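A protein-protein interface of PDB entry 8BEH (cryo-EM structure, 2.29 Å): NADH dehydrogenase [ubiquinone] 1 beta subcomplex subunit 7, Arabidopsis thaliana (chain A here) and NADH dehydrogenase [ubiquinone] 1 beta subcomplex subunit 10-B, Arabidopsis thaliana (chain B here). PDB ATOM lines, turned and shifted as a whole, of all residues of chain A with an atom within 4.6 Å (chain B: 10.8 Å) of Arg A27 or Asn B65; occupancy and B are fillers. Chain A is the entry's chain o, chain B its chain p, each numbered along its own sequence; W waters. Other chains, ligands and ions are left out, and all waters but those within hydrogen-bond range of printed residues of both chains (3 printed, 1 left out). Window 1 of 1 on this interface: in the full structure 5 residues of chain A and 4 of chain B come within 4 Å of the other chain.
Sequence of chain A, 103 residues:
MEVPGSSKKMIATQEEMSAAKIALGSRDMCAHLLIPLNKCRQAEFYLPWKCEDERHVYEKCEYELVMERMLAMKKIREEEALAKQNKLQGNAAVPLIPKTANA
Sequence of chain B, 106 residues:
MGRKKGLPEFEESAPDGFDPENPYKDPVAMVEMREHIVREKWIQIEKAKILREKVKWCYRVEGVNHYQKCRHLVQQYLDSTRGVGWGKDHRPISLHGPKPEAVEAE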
ATOM      1  N   MET A  17      10.961 -33.548   4.186  1.00  0.00           N
ATOM      2  CA  MET A  17      11.112 -32.599   5.283  1.00  0.00           C
ATOM      3  C   MET A  17      11.902 -31.370   4.852  1.00  0.00           C
ATOM      4  O   MET A  17      11.600 -30.254   5.286  1.00  0.00           O
ATOM      5  CB  MET A  17      11.768 -33.280   6.483  1.00  0.00           C
ATOM      6  CG  MET A  17      10.819 -34.210   7.225  1.00  0.00           C
ATOM      7  SD  MET A  17      11.494 -34.898   8.739  1.00  0.00           S
ATOM      8  CE  MET A  17      12.920 -35.770   8.113  1.00  0.00           C
ATOM      9  N   SER A  18      12.917 -31.554   3.999  1.00  0.00           N
ATOM     10  CA  SER A  18      13.662 -30.407   3.484  1.00  0.00           C
ATOM     11  C   SER A  18      12.812 -29.566   2.538  1.00  0.00           C
ATOM     12  O   SER A  18      12.879 -28.332   2.568  1.00  0.00           O
ATOM     13  CB  SER A  18      14.933 -30.874   2.776  1.00  0.00           C
ATOM     14  OG  SER A  18      15.924 -31.267   3.702  1.00  0.00           O
ATOM     15  N   LYS A  21      10.481 -27.388   4.374  1.00  0.00           N
ATOM     16  CA  LYS A  21      11.245 -26.436   5.259  1.00  0.00           C
ATOM     17  C   LYS A  21      10.880 -26.573   6.738  1.00  0.00           C
ATOM     18  O   LYS A  21      10.710 -25.561   7.349  1.00  0.00           O
ATOM     19  CB  LYS A  21      11.150 -25.019   4.666  1.00  0.00           C
ATOM     20  CG  LYS A  21      12.114 -24.774   3.518  1.00  0.00           C
ATOM     21  CD  LYS A  21      11.576 -23.924   2.402  1.00  0.00           C
ATOM     22  CE  LYS A  21      11.614 -22.444   2.686  1.00  0.00           C
ATOM     23  NZ  LYS A  21      11.784 -21.659   1.440  1.00  0.00           N
ATOM     24  N   ILE A  22      10.878 -27.791   7.273  1.00  0.00           N
ATOM     25  CA  ILE A  22      10.605 -28.015   8.711  1.00  0.00           C
ATOM     26  C   ILE A  22      11.793 -27.578   9.565  1.00  0.00           C
ATOM     27  O   ILE A  22      12.862 -27.996   9.279  1.00  0.00           O
ATOM     28  CB  ILE A  22      10.265 -29.506   9.019  1.00  0.00           C
ATOM     29  CG1 ILE A  22       9.334 -30.135   7.975  1.00  0.00           C
ATOM     30  CG2 ILE A  22       9.747 -29.662  10.425  1.00  0.00           C
ATOM     31  CD1 ILE A  22       8.018 -29.437   7.812  1.00  0.00           C
ATOM     32  N   ALA A  23      11.531 -26.800  10.598  1.00  0.00           N
ATOM     33  CA  ALA A  23      12.522 -26.457  11.615  1.00  0.00           C
ATOM     34  C   ALA A  23      13.134 -27.769  12.078  1.00  0.00           C
ATOM     35  O   ALA A  23      12.367 -28.750  12.308  1.00  0.00           O
ATOM     36  CB  ALA A  23      11.794 -25.756  12.717  1.00  0.00           C
ATOM     37  N   LEU A  24      14.446 -27.805  12.242  1.00  0.00           N
ATOM     38  CA  LEU A  24      15.158 -29.053  12.526  1.00  0.00           C
ATOM     39  C   LEU A  24      14.570 -29.784  13.738  1.00  0.00           C
ATOM     40  O   LEU A  24      14.561 -30.979  13.677  1.00  0.00           O
ATOM     41  CB  LEU A  24      16.641 -28.695  12.710  1.00  0.00           C
ATOM     42  CG  LEU A  24      17.348 -28.165  11.459  1.00  0.00           C
ATOM     43  CD1 LEU A  24      18.817 -27.905  11.732  1.00  0.00           C
ATOM     44  CD2 LEU A  24      17.181 -29.081  10.251  1.00  0.00           C
ATOM     45  N   GLY A  25      14.173 -29.070  14.803  1.00  0.00           N
ATOM     46  CA  GLY A  25      13.586 -29.658  15.996  1.00  0.00           C
ATOM     47  C   GLY A  25      12.196 -30.236  15.818  1.00  0.00           C
ATOM     48  O   GLY A  25      11.749 -30.836  16.706  1.00  0.00           O
ATOM     49  N   SER A  26      11.564 -30.032  14.702  1.00  0.00           N
ATOM     50  CA  SER A  26      10.248 -30.645  14.386  1.00  0.00           C
ATOM     51  C   SER A  26      10.465 -31.685  13.262  1.00  0.00           C
ATOM     52  O   SER A  26       9.551 -31.916  12.515  1.00  0.00           O
ATOM     53  CB  SER A  26       9.276 -29.563  14.108  1.00  0.00           C
ATOM     54  OG  SER A  26       9.067 -28.745  15.226  1.00  0.00           O
ATOM     55  N   ARG A  27      11.665 -32.252  13.140  1.00  0.00           N
ATOM     56  CA  ARG A  27      11.909 -33.364  12.169  1.00  0.00           C
ATOM     57  C   ARG A  27      11.906 -34.707  12.935  1.00  0.00           C
ATOM     58  O   ARG A  27      12.875 -35.395  12.904  1.00  0.00           O
ATOM     59  CB  ARG A  27      13.117 -33.081  11.269  1.00  0.00           C
ATOM     60  CG  ARG A  27      13.019 -31.837  10.408  1.00  0.00           C
ATOM     61  CD  ARG A  27      14.146 -31.729   9.407  1.00  0.00           C
ATOM     62  NE  ARG A  27      13.872 -30.602   8.546  1.00  0.00           N
ATOM     63  CZ  ARG A  27      14.591 -30.215   7.499  1.00  0.00           C
ATOM     64  NH1 ARG A  27      15.672 -30.872   7.137  1.00  0.00           N
ATOM     65  NH2 ARG A  27      14.210 -29.162   6.808  1.00  0.00           N
ATOM     66  N   ASP A  28      10.848 -34.953  13.629  1.00  0.00           N
ATOM     67  CA  ASP A  28      10.745 -36.153  14.443  1.00  0.00           C
ATOM     68  C   ASP A  28       9.818 -37.166  13.727  1.00  0.00           C
ATOM     69  O   ASP A  28       9.505 -36.965  12.583  1.00  0.00           O
ATOM     70  CB  ASP A  28      10.369 -35.707  15.852  1.00  0.00           C
ATOM     71  CG  ASP A  28       9.029 -35.039  16.051  1.00  0.00           C
ATOM     72  OD1 ASP A  28       8.896 -34.373  17.076  1.00  0.00           O
ATOM     73  OD2 ASP A  28       8.143 -35.190  15.205  1.00  0.00           O
ATOM     74  N   MET A  29       9.345 -38.161  14.454  1.00  0.00           N
ATOM     75  CA  MET A  29       8.491 -39.172  13.840  1.00  0.00           C
ATOM     76  C   MET A  29       7.148 -38.623  13.376  1.00  0.00           C
ATOM     77  O   MET A  29       6.467 -39.282  12.587  1.00  0.00           O
ATOM     78  CB  MET A  29       8.241 -40.317  14.823  1.00  0.00           C
ATOM     79  CG  MET A  29       9.473 -41.087  15.220  1.00  0.00           C
ATOM     80  SD  MET A  29       9.775 -42.531  14.191  1.00  0.00           S
ATOM     81  CE  MET A  29      11.507 -42.303  13.818  1.00  0.00           C
ATOM     82  N   ALA A  31       6.502 -35.824  11.628  1.00  0.00           N
ATOM     83  CA  ALA A  31       6.627 -34.783  10.612  1.00  0.00           C
ATOM     84  C   ALA A  31       5.719 -35.029   9.414  1.00  0.00           C
ATOM     85  O   ALA A  31       5.291 -34.069   8.755  1.00  0.00           O
ATOM     86  CB  ALA A  31       8.084 -34.668  10.158  1.00  0.00           C
ATOM     87  N   VAL B  55      28.090 -17.889   0.786  1.00  0.00           N
ATOM     88  CA  VAL B  55      27.517 -18.280   2.087  1.00  0.00           C
ATOM     89  C   VAL B  55      26.320 -17.410   2.372  1.00  0.00           C
ATOM     90  O   VAL B  55      25.309 -18.009   2.661  1.00  0.00           O
ATOM     91  CB  VAL B  55      28.574 -18.299   3.219  1.00  0.00           C
ATOM     92  CG1 VAL B  55      27.991 -18.527   4.589  1.00  0.00           C
ATOM     93  CG2 VAL B  55      29.696 -19.276   2.920  1.00  0.00           C
ATOM     94  N   TRP B  57      24.252 -15.802   0.509  1.00  0.00           N
ATOM     95  CA  TRP B  57      23.109 -16.174  -0.361  1.00  0.00           C
ATOM     96  C   TRP B  57      22.592 -17.591  -0.135  1.00  0.00           C
ATOM     97  O   TRP B  57      21.417 -17.691  -0.138  1.00  0.00           O
ATOM     98  CB  TRP B  57      23.423 -15.822  -1.806  1.00  0.00           C
ATOM     99  CG  TRP B  57      23.323 -14.334  -1.937  1.00  0.00           C
ATOM    100  CD1 TRP B  57      24.345 -13.453  -2.138  1.00  0.00           C
ATOM    101  CD2 TRP B  57      22.143 -13.535  -1.743  1.00  0.00           C
ATOM    102  NE1 TRP B  57      23.873 -12.175  -2.132  1.00  0.00           N
ATOM    103  CE2 TRP B  57      22.527 -12.187  -1.902  1.00  0.00           C
ATOM    104  CE3 TRP B  57      20.799 -13.824  -1.481  1.00  0.00           C
ATOM    105  CZ2 TRP B  57      21.623 -11.133  -1.797  1.00  0.00           C
ATOM    106  CZ3 TRP B  57      19.906 -12.783  -1.380  1.00  0.00           C
ATOM    107  CH2 TRP B  57      20.309 -11.456  -1.548  1.00  0.00           C
ATOM    108  N   CYS B  58      23.454 -18.565   0.152  1.00  0.00           N
ATOM    109  CA  CYS B  58      23.008 -19.950   0.454  1.00  0.00           C
ATOM    110  C   CYS B  58      22.180 -19.935   1.749  1.00  0.00           C
ATOM    111  O   CYS B  58      21.066 -20.374   1.660  1.00  0.00           O
ATOM    112  CB  CYS B  58      24.184 -20.918   0.377  1.00  0.00           C
ATOM    113  SG  CYS B  58      23.803 -22.655   0.694  1.00  0.00           S
ATOM    114  N   TYR B  59      22.661 -19.326   2.840  1.00  0.00           N
ATOM    115  CA  TYR B  59      21.884 -19.108   4.068  1.00  0.00           C
ATOM    116  C   TYR B  59      20.517 -18.549   3.698  1.00  0.00           C
ATOM    117  O   TYR B  59      19.577 -19.156   4.136  1.00  0.00           O
ATOM    118  CB  TYR B  59      22.612 -18.262   5.133  1.00  0.00           C
ATOM    119  CG  TYR B  59      21.971 -18.168   6.480  1.00  0.00           C
ATOM    120  CD1 TYR B  59      22.251 -19.114   7.447  1.00  0.00           C
ATOM    121  CD2 TYR B  59      21.119 -17.124   6.787  1.00  0.00           C
ATOM    122  CE1 TYR B  59      21.690 -19.030   8.698  1.00  0.00           C
ATOM    123  CE2 TYR B  59      20.549 -17.024   8.040  1.00  0.00           C
ATOM    124  CZ  TYR B  59      20.836 -17.985   8.990  1.00  0.00           C
ATOM    125  OH  TYR B  59      20.300 -17.934  10.229  1.00  0.00           O
ATOM    126  N   ARG B  60      20.473 -17.449   2.966  1.00  0.00           N
ATOM    127  CA  ARG B  60      19.252 -16.746   2.580  1.00  0.00           C
ATOM    128  C   ARG B  60      18.366 -17.611   1.678  1.00  0.00           C
ATOM    129  O   ARG B  60      17.194 -17.516   1.780  1.00  0.00           O
ATOM    130  CB  ARG B  60      19.613 -15.429   1.882  1.00  0.00           C
ATOM    131  CG  ARG B  60      20.158 -14.365   2.823  1.00  0.00           C
ATOM    132  CD  ARG B  60      20.799 -13.170   2.165  1.00  0.00           C
ATOM    133  NE  ARG B  60      21.291 -12.250   3.177  1.00  0.00           N
ATOM    134  CZ  ARG B  60      21.669 -11.001   2.952  1.00  0.00           C
ATOM    135  NH1 ARG B  60      21.635 -10.494   1.737  1.00  0.00           N
ATOM    136  NH2 ARG B  60      22.084 -10.265   3.957  1.00  0.00           N
ATOM    137  N   VAL B  61      18.986 -18.316   0.755  1.00  0.00           N
ATOM    138  CA  VAL B  61      18.115 -19.051  -0.154  1.00  0.00           C
ATOM    139  C   VAL B  61      17.627 -20.349   0.482  1.00  0.00           C
ATOM    140  O   VAL B  61      16.461 -20.721   0.336  1.00  0.00           O
ATOM    141  CB  VAL B  61      18.837 -19.296  -1.494  1.00  0.00           C
ATOM    142  CG1 VAL B  61      18.200 -20.445  -2.262  1.00  0.00           C
ATOM    143  CG2 VAL B  61      18.831 -18.029  -2.338  1.00  0.00           C
ATOM    144  N   GLU B  62      18.489 -21.049   1.214  1.00  0.00           N
ATOM    145  CA  GLU B  62      18.156 -22.381   1.697  1.00  0.00           C
ATOM    146  C   GLU B  62      17.440 -22.402   3.041  1.00  0.00           C
ATOM    147  O   GLU B  62      16.907 -23.451   3.415  1.00  0.00           O
ATOM    148  CB  GLU B  62      19.420 -23.238   1.779  1.00  0.00           C
ATOM    149  CG  GLU B  62      20.193 -23.297   0.480  1.00  0.00           C
ATOM    150  CD  GLU B  62      19.533 -24.173  -0.573  1.00  0.00           C
ATOM    151  OE1 GLU B  62      18.372 -24.579  -0.393  1.00  0.00           O
ATOM    152  OE2 GLU B  62      20.185 -24.453  -1.595  1.00  0.00           O
ATOM    153  N   GLY B  63      17.413 -21.290   3.769  1.00  0.00           N
ATOM    154  CA  GLY B  63      16.666 -21.235   5.016  1.00  0.00           C
ATOM    155  C   GLY B  63      17.137 -22.267   6.022  1.00  0.00           C
ATOM    156  O   GLY B  63      18.330 -22.392   6.309  1.00  0.00           O
ATOM    157  N   VAL B  64      16.224 -22.945   6.694  1.00  0.00           N
ATOM    158  CA  VAL B  64      16.510 -24.072   7.642  1.00  0.00           C
ATOM    159  C   VAL B  64      17.309 -25.229   7.024  1.00  0.00           C
ATOM    160  O   VAL B  64      17.865 -25.954   7.801  1.00  0.00           O
ATOM    161  CB  VAL B  64      15.195 -24.575   8.300  1.00  0.00           C
ATOM    162  CG1 VAL B  64      14.523 -23.480   9.124  1.00  0.00           C
ATOM    163  CG2 VAL B  64      14.231 -25.155   7.271  1.00  0.00           C
ATOM    164  N   ASN B  65      17.433 -25.339   5.718  1.00  0.00           N
ATOM    165  CA  ASN B  65      18.285 -26.359   5.121  1.00  0.00           C
ATOM    166  C   ASN B  65      19.720 -25.880   4.909  1.00  0.00           C
ATOM    167  O   ASN B  65      20.511 -26.587   4.276  1.00  0.00           O
ATOM    168  CB  ASN B  65      17.694 -26.839   3.791  1.00  0.00           C
ATOM    169  CG  ASN B  65      16.262 -27.331   3.926  1.00  0.00           C
ATOM    170  OD1 ASN B  65      15.926 -28.047   4.863  1.00  0.00           O
ATOM    171  ND2 ASN B  65      15.417 -26.946   2.986  1.00  0.00           N
ATOM    172  N   HIS B  66      20.071 -24.703   5.435  1.00  0.00           N
ATOM    173  CA  HIS B  66      21.391 -24.133   5.183  1.00  0.00           C
ATOM    174  C   HIS B  66      22.511 -24.992   5.759  1.00  0.00           C
ATOM    175  O   HIS B  66      23.596 -25.052   5.177  1.00  0.00           O
ATOM    176  CB  HIS B  66      21.461 -22.710   5.740  1.00  0.00           C
ATOM    177  CG  HIS B  66      21.646 -22.648   7.222  1.00  0.00           C
ATOM    178  ND1 HIS B  66      22.878 -22.763   7.824  1.00  0.00           N
ATOM    179  CD2 HIS B  66      20.754 -22.468   8.224  1.00  0.00           C
ATOM    180  CE1 HIS B  66      22.736 -22.668   9.133  1.00  0.00           C
ATOM    181  NE2 HIS B  66      21.458 -22.487   9.401  1.00  0.00           N
ATOM    182  N   TYR B  67      22.269 -25.668   6.886  1.00  0.00           N
ATOM    183  CA  TYR B  67      23.315 -26.481   7.500  1.00  0.00           C
ATOM    184  C   TYR B  67      23.813 -27.557   6.546  1.00  0.00           C
ATOM    185  O   TYR B  67      25.020 -27.797   6.440  1.00  0.00           O
ATOM    186  CB  TYR B  67      22.801 -27.134   8.780  1.00  0.00           C
ATOM    187  CG  TYR B  67      22.784 -26.249  10.003  1.00  0.00           C
ATOM    188  CD1 TYR B  67      23.937 -25.623  10.457  1.00  0.00           C
ATOM    189  CD2 TYR B  67      21.611 -26.060  10.717  1.00  0.00           C
ATOM    190  CE1 TYR B  67      23.914 -24.822  11.586  1.00  0.00           C
ATOM    191  CE2 TYR B  67      21.577 -25.272  11.838  1.00  0.00           C
ATOM    192  CZ  TYR B  67      22.727 -24.653  12.270  1.00  0.00           C
ATOM    193  OH  TYR B  67      22.680 -23.865  13.393  1.00  0.00           O
ATOM    194  N   GLN B  68      22.897 -28.219   5.846  1.00  0.00           N
ATOM    195  CA  GLN B  68      23.276 -29.272   4.917  1.00  0.00           C
ATOM    196  C   GLN B  68      23.611 -28.731   3.535  1.00  0.00           C
ATOM    197  O   GLN B  68      24.445 -29.315   2.839  1.00  0.00           O
ATOM    198  CB  GLN B  68      22.156 -30.323   4.847  1.00  0.00           C
ATOM    199  CG  GLN B  68      21.954 -31.009   3.510  1.00  0.00           C
ATOM    200  CD  GLN B  68      20.942 -32.142   3.594  1.00  0.00           C
ATOM    201  OE1 GLN B  68      19.835 -31.966   4.104  1.00  0.00           O
ATOM    202  NE2 GLN B  68      21.323 -33.313   3.104  1.00  0.00           N
ATOM    203  N   LYS B  69      23.025 -27.601   3.137  1.00  0.00           N
ATOM    204  CA  LYS B  69      23.296 -27.060   1.811  1.00  0.00           C
ATOM    205  C   LYS B  69      24.531 -26.162   1.752  1.00  0.00           C
ATOM    206  O   LYS B  69      25.223 -26.160   0.731  1.00  0.00           O
ATOM    207  CB  LYS B  69      22.080 -26.288   1.292  1.00  0.00           C
ATOM    208  CG  LYS B  69      20.825 -27.139   1.148  1.00  0.00           C
ATOM    209  CD  LYS B  69      21.014 -28.225   0.105  1.00  0.00           C
ATOM    210  CE  LYS B  69      19.752 -29.043  -0.110  1.00  0.00           C
ATOM    211  NZ  LYS B  69      19.936 -30.127  -1.116  1.00  0.00           N
ATOM    212  N   CYS B  70      24.827 -25.397   2.805  1.00  0.00           N
ATOM    213  CA  CYS B  70      25.961 -24.473   2.799  1.00  0.00           C
ATOM    214  C   CYS B  70      27.267 -25.114   3.238  1.00  0.00           C
ATOM    215  O   CYS B  70      28.292 -24.429   3.256  1.00  0.00           O
ATOM    216  CB  CYS B  70      25.706 -23.268   3.718  1.00  0.00           C
ATOM    217  SG  CYS B  70      24.124 -22.440   3.583  1.00  0.00           S
ATOM    218  N   ARG B  71      27.254 -26.403   3.584  1.00  0.00           N
ATOM    219  CA  ARG B  71      28.371 -27.007   4.304  1.00  0.00           C
ATOM    220  C   ARG B  71      29.691 -26.835   3.556  1.00  0.00           C
ATOM    221  O   ARG B  71      30.695 -26.407   4.137  1.00  0.00           O
ATOM    222  CB  ARG B  71      28.065 -28.482   4.549  1.00  0.00           C
ATOM    223  CG  ARG B  71      29.205 -29.302   5.060  1.00  0.00           C
ATOM    224  CD  ARG B  71      28.682 -30.579   5.689  1.00  0.00           C
ATOM    225  NE  ARG B  71      29.516 -31.025   6.796  1.00  0.00           N
ATOM    226  CZ  ARG B  71      30.551 -31.841   6.659  1.00  0.00           C
ATOM    227  NH1 ARG B  71      30.917 -32.298   5.474  1.00  0.00           N
ATOM    228  NH2 ARG B  71      31.231 -32.209   7.739  1.00  0.00           N
ATOM    229  N   HIS B  72      29.699 -27.147   2.258  1.00  0.00           N
ATOM    230  CA  HIS B  72      30.924 -27.021   1.476  1.00  0.00           C
ATOM    231  C   HIS B  72      31.333 -25.559   1.307  1.00  0.00           C
ATOM    232  O   HIS B  72      32.522 -25.230   1.383  1.00  0.00           O
ATOM    233  CB  HIS B  72      30.756 -27.740   0.129  1.00  0.00           C
ATOM    234  CG  HIS B  72      29.909 -27.011  -0.872  1.00  0.00           C
ATOM    235  ND1 HIS B  72      28.745 -27.544  -1.378  1.00  0.00           N
ATOM    236  CD2 HIS B  72      30.097 -25.839  -1.524  1.00  0.00           C
ATOM    237  CE1 HIS B  72      28.223 -26.706  -2.257  1.00  0.00           C
ATOM    238  NE2 HIS B  72      29.023 -25.662  -2.361  1.00  0.00           N
ATOM    239  N   LEU B  73      30.363 -24.666   1.097  1.00  0.00           N
ATOM    240  CA  LEU B  73      30.680 -23.246   0.984  1.00  0.00           C
ATOM    241  C   LEU B  73      31.215 -22.697   2.298  1.00  0.00           C
ATOM    242  O   LEU B  73      32.157 -21.896   2.304  1.00  0.00           O
ATOM    243  CB  LEU B  73      29.448 -22.463   0.536  1.00  0.00           C
ATOM    244  CG  LEU B  73      29.055 -22.605  -0.933  1.00  0.00           C
ATOM    245  CD1 LEU B  73      27.857 -21.731  -1.257  1.00  0.00           C
ATOM    246  CD2 LEU B  73      30.229 -22.284  -1.847  1.00  0.00           C
ATOM    247  N   VAL B  74      30.627 -23.118   3.421  1.00  0.00           N
ATOM    248  CA  VAL B  74      31.109 -22.676   4.724  1.00  0.00           C
ATOM    249  C   VAL B  74      32.538 -23.150   4.944  1.00  0.00           C
ATOM    250  O   VAL B  74      33.392 -22.392   5.421  1.00  0.00           O
ATOM    251  CB  VAL B  74      30.172 -23.165   5.844  1.00  0.00           C
ATOM    252  CG1 VAL B  74      30.824 -22.982   7.207  1.00  0.00           C
ATOM    253  CG2 VAL B  74      28.846 -22.437   5.784  1.00  0.00           C
HETATM  254  O   HOH W   1      17.977 -29.699   2.354  1.00  0.00           O
HETATM  255  O   HOH W   2      14.630 -21.516   2.357  1.00  0.00           O
HETATM  256  O   HOH W   3      18.363 -30.081   5.603  1.00  0.00           O
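Among the printed residues, merely in contact across the chains: Ser A18 with Gln B68, Lys A21 with Val B64, Lys A21 with Asn B65, Ile A22 with Val B64 and Leu A24 with Tyr B67.
Of the 19 printed residues of chain B, 4 touch a printed residue of chain A.
Printed residues of chain B that touch a printed residue of chain A: Val B64, Asn B65, Tyr B67 and Gln B68.
Hydrophobic or aromatic side chains of chain B that line the printed part of chain A: Val B64 and Tyr B67.
Along chain B the printed residues that touch a printed residue of chain A span positions 64 to 68.
Of the 12 printed residues of chain A, 5 touch a printed residue of chain B.
Printed residues of chain A that touch a printed residue of chain B: Ser A18, Lys A21, Ile A22, Leu A24 and Arg A27.
Hydrophobic or aromatic side chains of chain A within 4 Å of the printed part of chain B: Leu A24.
Among the printed residues, no Asp or Glu carboxylate lies within 4 Å of a Lys or Arg side-chain nitrogen of the other chain.
No residue of chain B comes within 4 Å of Met A17.
Of the printed residues of chain B, Ser A18 touches Asn B65 and Gln B68.
Of the printed residues of chain B, Lys A21 touches Val B64 and Asn B65.
Ile A22 touches just one residue of chain B: Val B64 (3.7 Å).
No residue of chain B comes within 4 Å of Ala A23.
No residue of chain B comes within 4 Å of Gly A25.
Ser A26 touches none of the printed residues of chain B.
No residue of chain B comes within 4 Å of Asp A28.
Of the printed residues of chain A, Val B64 touches Lys A21 and Ile A22.
Of the printed residues of chain A, Asn B65 touches Ser A18 (2.9 Å), Lys A21 (3.99 Å) and Arg A27 (2.8 Å).
Printed residues of chain A within 4 Å of Tyr B67: Leu A24 (3.5 Å).
The nearest printed residue of chain A that does not touch Asn B65 is Met A17 (4.9 Å).
The nearest printed residue of chain A that does not touch Val B64 is Leu A24 (4.03 Å).
The side-chain amide oxygen (OD1) of Asn B65 lies within hydrogen-bond range of the guanidinium group (NH2) of Arg A27 (2.8 Å).
O of Ser A18 sits at hydrogen-bond distance from ND2 of Asn B65 (2.9 Å).
Water W3 lies within hydrogen-bond range of the side-chain amide oxygen of Gln B68, the guanidinium group of Arg A27, the side-chain amide oxygen of Asn B65 and the side-chain hydroxyl of Ser A18.
Water W2 lies within hydrogen-bond range of O of Val B61 (2.8 Å), NZ of Lys A21 (3.0 Å), N of Gly B63 (3.1 Å) and O of Glu B62 (3.2 Å).
Water W1 bridges OG of Ser A18 (2.9 Å) and OE1 of Gln B68 (3.4 Å).
The guanidinium group (NE) of Arg A27 lies within hydrogen-bond range of the backbone carbonyl oxygen (O) of Ile A22 (2.9 Å).
The guanidinium group (NH2) of Arg A27 is in hydrogen-bond range of the backbone carbonyl oxygen (O) of Met A17, at 3.2 Å.
The backbone carbonyl oxygen (O) of Met A17 is in hydrogen-bond range of the backbone NH (N) of Ile A22, at 3.2 Å.
NH1 of Arg A27 sits at hydrogen-bond distance from OG of Ser A18.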
